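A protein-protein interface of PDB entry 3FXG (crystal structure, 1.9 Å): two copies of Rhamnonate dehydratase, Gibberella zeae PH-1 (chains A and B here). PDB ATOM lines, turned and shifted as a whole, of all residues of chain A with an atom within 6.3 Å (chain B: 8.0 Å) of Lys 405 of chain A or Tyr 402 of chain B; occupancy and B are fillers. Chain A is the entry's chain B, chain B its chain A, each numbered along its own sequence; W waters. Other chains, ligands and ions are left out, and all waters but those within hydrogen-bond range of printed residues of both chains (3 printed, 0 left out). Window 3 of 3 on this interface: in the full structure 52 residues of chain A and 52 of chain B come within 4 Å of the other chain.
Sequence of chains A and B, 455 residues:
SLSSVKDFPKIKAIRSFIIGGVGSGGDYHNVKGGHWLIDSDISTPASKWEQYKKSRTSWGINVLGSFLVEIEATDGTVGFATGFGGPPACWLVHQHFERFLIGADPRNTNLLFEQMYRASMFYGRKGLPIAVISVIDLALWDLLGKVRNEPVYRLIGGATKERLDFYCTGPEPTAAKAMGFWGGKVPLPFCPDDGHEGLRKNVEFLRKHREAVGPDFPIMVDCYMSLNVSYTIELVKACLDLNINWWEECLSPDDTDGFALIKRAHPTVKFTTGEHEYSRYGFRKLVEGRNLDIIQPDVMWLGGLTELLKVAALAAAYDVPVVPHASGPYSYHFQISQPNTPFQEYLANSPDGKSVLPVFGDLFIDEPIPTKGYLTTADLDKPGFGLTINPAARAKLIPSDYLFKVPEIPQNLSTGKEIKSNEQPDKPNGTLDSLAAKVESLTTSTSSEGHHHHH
Printed residues of chain B that touch a printed residue of chain A: Pro 87, Pro 88, Ile 398, Tyr 402, Leu 403, Lys 405 and Pro 407. Hydrophobic or aromatic side chains of chain B that line the printed part of chain A: Pro 87, Pro 88, Ile 398, Tyr 402, Leu 403 and Pro 407. Printed residues of chain A that touch a printed residue of chain B: Trp 91, Tyr 402, Leu 403, Lys 405, Val 406 and Pro 407. Among the printed residues, 11 pairs touch across the chains.
Tyr 402 of chain A touches Leu 403 of chain B, and with the chains exchanged Leu 403 of chain A touches Tyr 402 of chain B. Tyr 402 of chain A touches Lys 405 of chain B, and with the chains exchanged Lys 405 of chain A touches Tyr 402 of chain B. Tyr 402 of chain A touches Pro 407 of chain B, and with the chains exchanged Pro 407 of chain A touches Tyr 402 of chain B. Leu 403 of chain A touches its own counterpart, Leu 403 of chain B. Of the 11 pairs that touch across the chains among the printed residues, 7 have their exchanged pair printed and touching as well.
NE1 of Trp 91 of chain A touches CB of Pro 87 of chain B, at 3.5 Å. Trp 91 of chain A touches Pro 88 of chain B. Tyr 402 of chain A touches Leu 403 of chain B (CE1 to O, 3.6 Å). Pro 407 of chain B touches Tyr 402 of chain A (CD to CD2, 3.6 Å). Leu 403 of chain A touches Tyr 402 of chain B. O of Leu 403 of chain B touches CD2 of Leu 403 of chain A, at 3.8 Å. CD1 of Tyr 402 of chain B touches O of Lys 405 of chain A, at 3.5 Å. Val 406 of chain A touches Ile 398 of chain B (CG2 to CD1, 3.7 Å). Ile 398 of chain B touches Pro 407 of chain A. Tyr 402 of chain B touches Pro 407 of chain A.
Printed residues of chain B within 4 Å of Trp 91 of chain A: Pro 87 (3.5 Å) and Pro 88 (3.7 Å). Of the printed residues of chain B, Leu 403 of chain A touches Tyr 402 (3.6 Å) and Leu 403 (3.8 Å). Of the printed residues of chain B, Lys 405 of chain A touches Tyr 402 (3.5 Å). Of the printed residues of chain B, Val 406 of chain A touches Ile 398. Asp 401 of chain B touches none of the printed residues of chain A. Tyr 402 of chain B touches just these residues of chain A: Leu 403 (3.6 Å), Lys 405 (3.5 Å) and Pro 407 (3.6 Å). Of the printed residues of chain A, Lys 405 of chain B touches Tyr 402 (3.5 Å). Of the printed residues of chain A, Pro 407 of chain B touches Tyr 402 (3.6 Å). The nearest residue of chain A that does not touch Tyr 402 of chain B is Val 406 of chain A (4.1 Å).
Water W2 lies within hydrogen-bond range of OH of Tyr 402 of chain B (2.6 Å), O of Leu 403 of chain A (2.7 Å) and NE1 of Trp 91 of chain A (3.2 Å). Water W1 lies within hydrogen-bond range of OH of Tyr 402 of chain A, O of Leu 403 of chain B and NE1 of Trp 91 of chain B. Water W3 bridges O of Tyr 402 of chain A (2.7 Å) and O of Tyr 402 of chain B (2.8 Å).
The backbone NH (N) of Ile 18 of chain B lies within hydrogen-bond range of the backbone carbonyl oxygen (O) of Ile 398 of chain B, at 2.8 Å.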
ATOM      1  N   TRP A  91      17.369  -0.751  -6.869  1.00  0.00           N
ATOM      2  CA  TRP A  91      16.801  -1.612  -7.897  1.00  0.00           C
ATOM      3  C   TRP A  91      17.746  -2.778  -8.186  1.00  0.00           C
ATOM      4  O   TRP A  91      17.325  -3.931  -8.244  1.00  0.00           O
ATOM      5  CB  TRP A  91      16.565  -0.821  -9.186  1.00  0.00           C
ATOM      6  CG  TRP A  91      15.679  -1.536 -10.166  1.00  0.00           C
ATOM      7  CD1 TRP A  91      14.317  -1.463 -10.242  1.00  0.00           C
ATOM      8  CD2 TRP A  91      16.089  -2.465 -11.180  1.00  0.00           C
ATOM      9  NE1 TRP A  91      13.852  -2.289 -11.241  1.00  0.00           N
ATOM     10  CE2 TRP A  91      14.920  -2.917 -11.831  1.00  0.00           C
ATOM     11  CE3 TRP A  91      17.331  -2.963 -11.599  1.00  0.00           C
ATOM     12  CZ2 TRP A  91      14.955  -3.843 -12.883  1.00  0.00           C
ATOM     13  CZ3 TRP A  91      17.365  -3.885 -12.644  1.00  0.00           C
ATOM     14  CH2 TRP A  91      16.182  -4.314 -13.273  1.00  0.00           C
ATOM     15  N   ASP A 401      10.518  -0.852  -2.147  1.00  0.00           N
ATOM     16  CA  ASP A 401       9.439  -1.646  -2.734  1.00  0.00           C
ATOM     17  C   ASP A 401       8.725  -1.017  -3.930  1.00  0.00           C
ATOM     18  O   ASP A 401       8.415  -1.706  -4.899  1.00  0.00           O
ATOM     19  CB  ASP A 401       8.398  -1.984  -1.664  1.00  0.00           C
ATOM     20  CG  ASP A 401       8.970  -2.816  -0.538  1.00  0.00           C
ATOM     21  OD1 ASP A 401       8.196  -3.217   0.354  1.00  0.00           O
ATOM     22  OD2 ASP A 401      10.194  -3.069  -0.543  1.00  0.00           O
ATOM     23  N   TYR A 402       8.461   0.283  -3.861  1.00  0.00           N
ATOM     24  CA  TYR A 402       7.752   0.979  -4.934  1.00  0.00           C
ATOM     25  C   TYR A 402       8.430   0.874  -6.302  1.00  0.00           C
ATOM     26  O   TYR A 402       7.773   0.971  -7.341  1.00  0.00           O
ATOM     27  CB  TYR A 402       7.561   2.454  -4.558  1.00  0.00           C
ATOM     28  CG  TYR A 402       8.788   3.323  -4.748  1.00  0.00           C
ATOM     29  CD1 TYR A 402       8.992   4.020  -5.938  1.00  0.00           C
ATOM     30  CD2 TYR A 402       9.749   3.443  -3.743  1.00  0.00           C
ATOM     31  CE1 TYR A 402      10.122   4.819  -6.126  1.00  0.00           C
ATOM     32  CE2 TYR A 402      10.884   4.239  -3.921  1.00  0.00           C
ATOM     33  CZ  TYR A 402      11.063   4.922  -5.115  1.00  0.00           C
ATOM     34  OH  TYR A 402      12.182   5.704  -5.301  1.00  0.00           O
ATOM     35  N   LEU A 403       9.744   0.673  -6.304  1.00  0.00           N
ATOM     36  CA  LEU A 403      10.496   0.571  -7.552  1.00  0.00           C
ATOM     37  C   LEU A 403      10.211  -0.711  -8.315  1.00  0.00           C
ATOM     38  O   LEU A 403      10.572  -0.836  -9.488  1.00  0.00           O
ATOM     39  CB  LEU A 403      11.996   0.666  -7.264  1.00  0.00           C
ATOM     40  CG  LEU A 403      12.477   2.024  -6.751  1.00  0.00           C
ATOM     41  CD1 LEU A 403      13.890   1.906  -6.196  1.00  0.00           C
ATOM     42  CD2 LEU A 403      12.420   3.034  -7.886  1.00  0.00           C
ATOM     43  N   PHE A 404       9.561  -1.661  -7.653  1.00  0.00           N
ATOM     44  CA  PHE A 404       9.253  -2.935  -8.282  1.00  0.00           C
ATOM     45  C   PHE A 404       7.763  -3.115  -8.557  1.00  0.00           C
ATOM     46  O   PHE A 404       7.328  -4.183  -8.976  1.00  0.00           O
ATOM     47  CB  PHE A 404       9.782  -4.067  -7.401  1.00  0.00           C
ATOM     48  CG  PHE A 404      11.227  -3.898  -7.018  1.00  0.00           C
ATOM     49  CD1 PHE A 404      12.229  -3.949  -7.985  1.00  0.00           C
ATOM     50  CD2 PHE A 404      11.584  -3.648  -5.699  1.00  0.00           C
ATOM     51  CE1 PHE A 404      13.562  -3.750  -7.642  1.00  0.00           C
ATOM     52  CE2 PHE A 404      12.915  -3.448  -5.344  1.00  0.00           C
ATOM     53  CZ  PHE A 404      13.907  -3.498  -6.317  1.00  0.00           C
ATOM     54  N   LYS A 405       6.988  -2.061  -8.321  1.00  0.00           N
ATOM     55  CA  LYS A 405       5.548  -2.095  -8.557  1.00  0.00           C
ATOM     56  C   LYS A 405       5.270  -1.698 -10.005  1.00  0.00           C
ATOM     57  O   LYS A 405       4.754  -0.612 -10.270  1.00  0.00           O
ATOM     58  CB  LYS A 405       4.830  -1.120  -7.618  1.00  0.00           C
ATOM     59  CG  LYS A 405       4.923  -1.460  -6.136  1.00  0.00           C
ATOM     60  CD  LYS A 405       4.255  -2.788  -5.823  1.00  0.00           C
ATOM     61  CE  LYS A 405       3.953  -2.924  -4.334  1.00  0.00           C
ATOM     62  NZ  LYS A 405       5.170  -2.833  -3.481  1.00  0.00           N
ATOM     63  N   VAL A 406       5.616  -2.578 -10.938  1.00  0.00           N
ATOM     64  CA  VAL A 406       5.411  -2.297 -12.353  1.00  0.00           C
ATOM     65  C   VAL A 406       3.945  -2.461 -12.753  1.00  0.00           C
ATOM     66  O   VAL A 406       3.311  -3.466 -12.434  1.00  0.00           O
ATOM     67  CB  VAL A 406       6.295  -3.214 -13.238  1.00  0.00           C
ATOM     68  CG1 VAL A 406       5.898  -4.665 -13.052  1.00  0.00           C
ATOM     69  CG2 VAL A 406       6.173  -2.809 -14.698  1.00  0.00           C
ATOM     70  N   PRO A 407       3.384  -1.461 -13.450  1.00  0.00           N
ATOM     71  CA  PRO A 407       1.985  -1.510 -13.887  1.00  0.00           C
ATOM     72  C   PRO A 407       1.704  -2.629 -14.886  1.00  0.00           C
ATOM     73  O   PRO A 407       2.594  -3.055 -15.621  1.00  0.00           O
ATOM     74  CB  PRO A 407       1.763  -0.122 -14.484  1.00  0.00           C
ATOM     75  CG  PRO A 407       3.120   0.243 -14.998  1.00  0.00           C
ATOM     76  CD  PRO A 407       4.019  -0.200 -13.872  1.00  0.00           C
ATOM     77  N   PHE B  17      10.349   4.201 -22.010  1.00  0.00           N
ATOM     78  CA  PHE B  17       9.464   3.085 -21.718  1.00  0.00           C
ATOM     79  C   PHE B  17      10.262   1.824 -21.457  1.00  0.00           C
ATOM     80  O   PHE B  17      11.340   1.630 -22.017  1.00  0.00           O
ATOM     81  CB  PHE B  17       8.548   2.812 -22.914  1.00  0.00           C
ATOM     82  CG  PHE B  17       7.709   3.981 -23.322  1.00  0.00           C
ATOM     83  CD1 PHE B  17       6.447   4.173 -22.771  1.00  0.00           C
ATOM     84  CD2 PHE B  17       8.185   4.900 -24.253  1.00  0.00           C
ATOM     85  CE1 PHE B  17       5.667   5.264 -23.142  1.00  0.00           C
ATOM     86  CE2 PHE B  17       7.413   5.996 -24.632  1.00  0.00           C
ATOM     87  CZ  PHE B  17       6.151   6.178 -24.074  1.00  0.00           C
ATOM     88  N   ILE B  18       9.722   0.966 -20.604  1.00  0.00           N
ATOM     89  CA  ILE B  18      10.349  -0.313 -20.319  1.00  0.00           C
ATOM     90  C   ILE B  18       9.596  -1.288 -21.216  1.00  0.00           C
ATOM     91  O   ILE B  18       8.372  -1.208 -21.326  1.00  0.00           O
ATOM     92  CB  ILE B  18      10.152  -0.721 -18.853  1.00  0.00           C
ATOM     93  CG1 ILE B  18      10.889   0.268 -17.947  1.00  0.00           C
ATOM     94  CG2 ILE B  18      10.648  -2.145 -18.637  1.00  0.00           C
ATOM     95  CD1 ILE B  18      10.524   0.152 -16.493  1.00  0.00           C
ATOM     96  N   GLY B  86      16.659  -1.329 -19.100  1.00  0.00           N
ATOM     97  CA  GLY B  86      15.391  -1.375 -18.395  1.00  0.00           C
ATOM     98  C   GLY B  86      15.064  -0.234 -17.453  1.00  0.00           C
ATOM     99  O   GLY B  86      15.362   0.923 -17.743  1.00  0.00           O
ATOM    100  N   PRO B  87      14.445  -0.539 -16.302  1.00  0.00           N
ATOM    101  CA  PRO B  87      14.058   0.451 -15.291  1.00  0.00           C
ATOM    102  C   PRO B  87      15.159   1.413 -14.836  1.00  0.00           C
ATOM    103  O   PRO B  87      14.975   2.629 -14.870  1.00  0.00           O
ATOM    104  CB  PRO B  87      13.526  -0.416 -14.149  1.00  0.00           C
ATOM    105  CG  PRO B  87      12.946  -1.586 -14.868  1.00  0.00           C
ATOM    106  CD  PRO B  87      14.013  -1.888 -15.899  1.00  0.00           C
ATOM    107  N   PRO B  88      16.316   0.889 -14.401  1.00  0.00           N
ATOM    108  CA  PRO B  88      17.368   1.815 -13.963  1.00  0.00           C
ATOM    109  C   PRO B  88      17.819   2.777 -15.062  1.00  0.00           C
ATOM    110  O   PRO B  88      18.192   3.918 -14.784  1.00  0.00           O
ATOM    111  CB  PRO B  88      18.479   0.878 -13.482  1.00  0.00           C
ATOM    112  CG  PRO B  88      18.271  -0.361 -14.306  1.00  0.00           C
ATOM    113  CD  PRO B  88      16.768  -0.510 -14.305  1.00  0.00           C
ATOM    114  N   CYS B  90      15.869   3.964 -17.516  1.00  0.00           N
ATOM    115  CA  CYS B  90      14.820   4.972 -17.642  1.00  0.00           C
ATOM    116  C   CYS B  90      14.885   5.993 -16.518  1.00  0.00           C
ATOM    117  O   CYS B  90      14.618   7.174 -16.730  1.00  0.00           O
ATOM    118  CB  CYS B  90      13.436   4.315 -17.644  1.00  0.00           C
ATOM    119  SG  CYS B  90      13.104   3.300 -19.098  1.00  0.00           S
ATOM    120  N   TRP B  91      15.236   5.533 -15.322  1.00  0.00           N
ATOM    121  CA  TRP B  91      15.335   6.424 -14.170  1.00  0.00           C
ATOM    122  C   TRP B  91      16.396   7.486 -14.445  1.00  0.00           C
ATOM    123  O   TRP B  91      16.179   8.672 -14.199  1.00  0.00           O
ATOM    124  CB  TRP B  91      15.719   5.630 -12.922  1.00  0.00           C
ATOM    125  CG  TRP B  91      15.541   6.385 -11.641  1.00  0.00           C
ATOM    126  CD1 TRP B  91      14.437   6.386 -10.833  1.00  0.00           C
ATOM    127  CD2 TRP B  91      16.499   7.246 -11.012  1.00  0.00           C
ATOM    128  NE1 TRP B  91      14.651   7.189  -9.739  1.00  0.00           N
ATOM    129  CE2 TRP B  91      15.908   7.730  -9.823  1.00  0.00           C
ATOM    130  CE3 TRP B  91      17.803   7.655 -11.339  1.00  0.00           C
ATOM    131  CZ2 TRP B  91      16.575   8.605  -8.954  1.00  0.00           C
ATOM    132  CZ3 TRP B  91      18.468   8.527 -10.475  1.00  0.00           C
ATOM    133  CH2 TRP B  91      17.850   8.991  -9.294  1.00  0.00           C
ATOM    134  N   ILE B 398       5.779  -0.032 -21.297  1.00  0.00           N
ATOM    135  CA  ILE B 398       5.460   0.421 -19.954  1.00  0.00           C
ATOM    136  C   ILE B 398       6.074   1.784 -19.657  1.00  0.00           C
ATOM    137  O   ILE B 398       7.296   1.914 -19.579  1.00  0.00           O
ATOM    138  CB  ILE B 398       5.986  -0.587 -18.912  1.00  0.00           C
ATOM    139  CG1 ILE B 398       5.465  -1.987 -19.242  1.00  0.00           C
ATOM    140  CG2 ILE B 398       5.559  -0.170 -17.520  1.00  0.00           C
ATOM    141  CD1 ILE B 398       6.086  -3.083 -18.405  1.00  0.00           C
ATOM    142  N   PRO B 399       5.236   2.821 -19.495  1.00  0.00           N
ATOM    143  CA  PRO B 399       5.760   4.158 -19.199  1.00  0.00           C
ATOM    144  C   PRO B 399       6.620   4.060 -17.936  1.00  0.00           C
ATOM    145  O   PRO B 399       6.268   3.344 -16.999  1.00  0.00           O
ATOM    146  CB  PRO B 399       4.493   4.981 -18.975  1.00  0.00           C
ATOM    147  CG  PRO B 399       3.504   4.315 -19.882  1.00  0.00           C
ATOM    148  CD  PRO B 399       3.769   2.850 -19.621  1.00  0.00           C
ATOM    149  N   SER B 400       7.743   4.769 -17.914  1.00  0.00           N
ATOM    150  CA  SER B 400       8.643   4.719 -16.765  1.00  0.00           C
ATOM    151  C   SER B 400       8.168   5.555 -15.579  1.00  0.00           C
ATOM    152  O   SER B 400       8.828   5.595 -14.540  1.00  0.00           O
ATOM    153  CB  SER B 400      10.043   5.172 -17.185  1.00  0.00           C
ATOM    154  OG  SER B 400      10.017   6.493 -17.692  1.00  0.00           O
ATOM    155  N   ASP B 401       7.017   6.205 -15.742  1.00  0.00           N
ATOM    156  CA  ASP B 401       6.424   7.060 -14.712  1.00  0.00           C
ATOM    157  C   ASP B 401       6.391   6.476 -13.297  1.00  0.00           C
ATOM    158  O   ASP B 401       6.667   7.180 -12.326  1.00  0.00           O
ATOM    159  CB  ASP B 401       4.995   7.439 -15.121  1.00  0.00           C
ATOM    160  CG  ASP B 401       4.951   8.297 -16.376  1.00  0.00           C
ATOM    161  OD1 ASP B 401       5.697   8.009 -17.336  1.00  0.00           O
ATOM    162  OD2 ASP B 401       4.155   9.257 -16.406  1.00  0.00           O
ATOM    163  N   TYR B 402       6.049   5.197 -13.178  1.00  0.00           N
ATOM    164  CA  TYR B 402       5.955   4.560 -11.867  1.00  0.00           C
ATOM    165  C   TYR B 402       7.248   4.620 -11.055  1.00  0.00           C
ATOM    166  O   TYR B 402       7.213   4.632  -9.826  1.00  0.00           O
ATOM    167  CB  TYR B 402       5.507   3.100 -12.024  1.00  0.00           C
ATOM    168  CG  TYR B 402       6.587   2.145 -12.482  1.00  0.00           C
ATOM    169  CD1 TYR B 402       7.341   1.418 -11.557  1.00  0.00           C
ATOM    170  CD2 TYR B 402       6.857   1.962 -13.838  1.00  0.00           C
ATOM    171  CE1 TYR B 402       8.333   0.530 -11.972  1.00  0.00           C
ATOM    172  CE2 TYR B 402       7.848   1.077 -14.263  1.00  0.00           C
ATOM    173  CZ  TYR B 402       8.580   0.367 -13.327  1.00  0.00           C
ATOM    174  OH  TYR B 402       9.560  -0.505 -13.743  1.00  0.00           O
ATOM    175  N   LEU B 403       8.384   4.664 -11.744  1.00  0.00           N
ATOM    176  CA  LEU B 403       9.683   4.708 -11.079  1.00  0.00           C
ATOM    177  C   LEU B 403       9.924   5.999 -10.302  1.00  0.00           C
ATOM    178  O   LEU B 403      10.831   6.070  -9.468  1.00  0.00           O
ATOM    179  CB  LEU B 403      10.800   4.520 -12.111  1.00  0.00           C
ATOM    180  CG  LEU B 403      10.924   3.135 -12.747  1.00  0.00           C
ATOM    181  CD1 LEU B 403      11.857   3.201 -13.947  1.00  0.00           C
ATOM    182  CD2 LEU B 403      11.439   2.142 -11.712  1.00  0.00           C
ATOM    183  N   PHE B 404       9.110   7.013 -10.568  1.00  0.00           N
ATOM    184  CA  PHE B 404       9.270   8.299  -9.906  1.00  0.00           C
ATOM    185  C   PHE B 404       8.187   8.597  -8.876  1.00  0.00           C
ATOM    186  O   PHE B 404       8.161   9.678  -8.290  1.00  0.00           O
ATOM    187  CB  PHE B 404       9.321   9.399 -10.964  1.00  0.00           C
ATOM    188  CG  PHE B 404      10.319   9.129 -12.056  1.00  0.00           C
ATOM    189  CD1 PHE B 404      11.685   9.163 -11.794  1.00  0.00           C
ATOM    190  CD2 PHE B 404       9.893   8.800 -13.339  1.00  0.00           C
ATOM    191  CE1 PHE B 404      12.612   8.873 -12.795  1.00  0.00           C
ATOM    192  CE2 PHE B 404      10.809   8.509 -14.345  1.00  0.00           C
ATOM    193  CZ  PHE B 404      12.171   8.544 -14.074  1.00  0.00           C
ATOM    194  N   LYS B 405       7.296   7.636  -8.654  1.00  0.00           N
ATOM    195  CA  LYS B 405       6.226   7.800  -7.675  1.00  0.00           C
ATOM    196  C   LYS B 405       6.722   7.390  -6.293  1.00  0.00           C
ATOM    197  O   LYS B 405       6.343   6.341  -5.769  1.00  0.00           O
ATOM    198  CB  LYS B 405       5.010   6.951  -8.059  1.00  0.00           C
ATOM    199  CG  LYS B 405       4.001   7.659  -8.954  1.00  0.00           C
ATOM    200  CD  LYS B 405       4.618   8.116 -10.262  1.00  0.00           C
ATOM    201  CE  LYS B 405       3.628   8.933 -11.080  1.00  0.00           C
ATOM    202  NZ  LYS B 405       2.402   8.160 -11.412  1.00  0.00           N
ATOM    203  N   VAL B 406       7.576   8.223  -5.710  1.00  0.00           N
ATOM    204  CA  VAL B 406       8.130   7.946  -4.392  1.00  0.00           C
ATOM    205  C   VAL B 406       7.083   8.186  -3.307  1.00  0.00           C
ATOM    206  O   VAL B 406       6.446   9.239  -3.264  1.00  0.00           O
ATOM    207  CB  VAL B 406       9.372   8.830  -4.116  1.00  0.00           C
ATOM    208  CG1 VAL B 406       9.027  10.294  -4.327  1.00  0.00           C
ATOM    209  CG2 VAL B 406       9.873   8.602  -2.698  1.00  0.00           C
ATOM    210  N   PRO B 407       6.883   7.199  -2.423  1.00  0.00           N
ATOM    211  CA  PRO B 407       5.898   7.345  -1.349  1.00  0.00           C
ATOM    212  C   PRO B 407       6.268   8.446  -0.363  1.00  0.00           C
ATOM    213  O   PRO B 407       7.443   8.767  -0.190  1.00  0.00           O
ATOM    214  CB  PRO B 407       5.882   5.958  -0.707  1.00  0.00           C
ATOM    215  CG  PRO B 407       7.275   5.466  -0.934  1.00  0.00           C
ATOM    216  CD  PRO B 407       7.542   5.883  -2.359  1.00  0.00           C
HETATM  217  O   HOH W   1      12.575   7.137  -7.535  1.00  0.00           O
HETATM  218  O   HOH W   2      10.809  -1.934 -11.982  1.00  0.00           O
HETATM  219  O   HOH W   3       5.941   2.848  -8.124  1.00  0.00           O
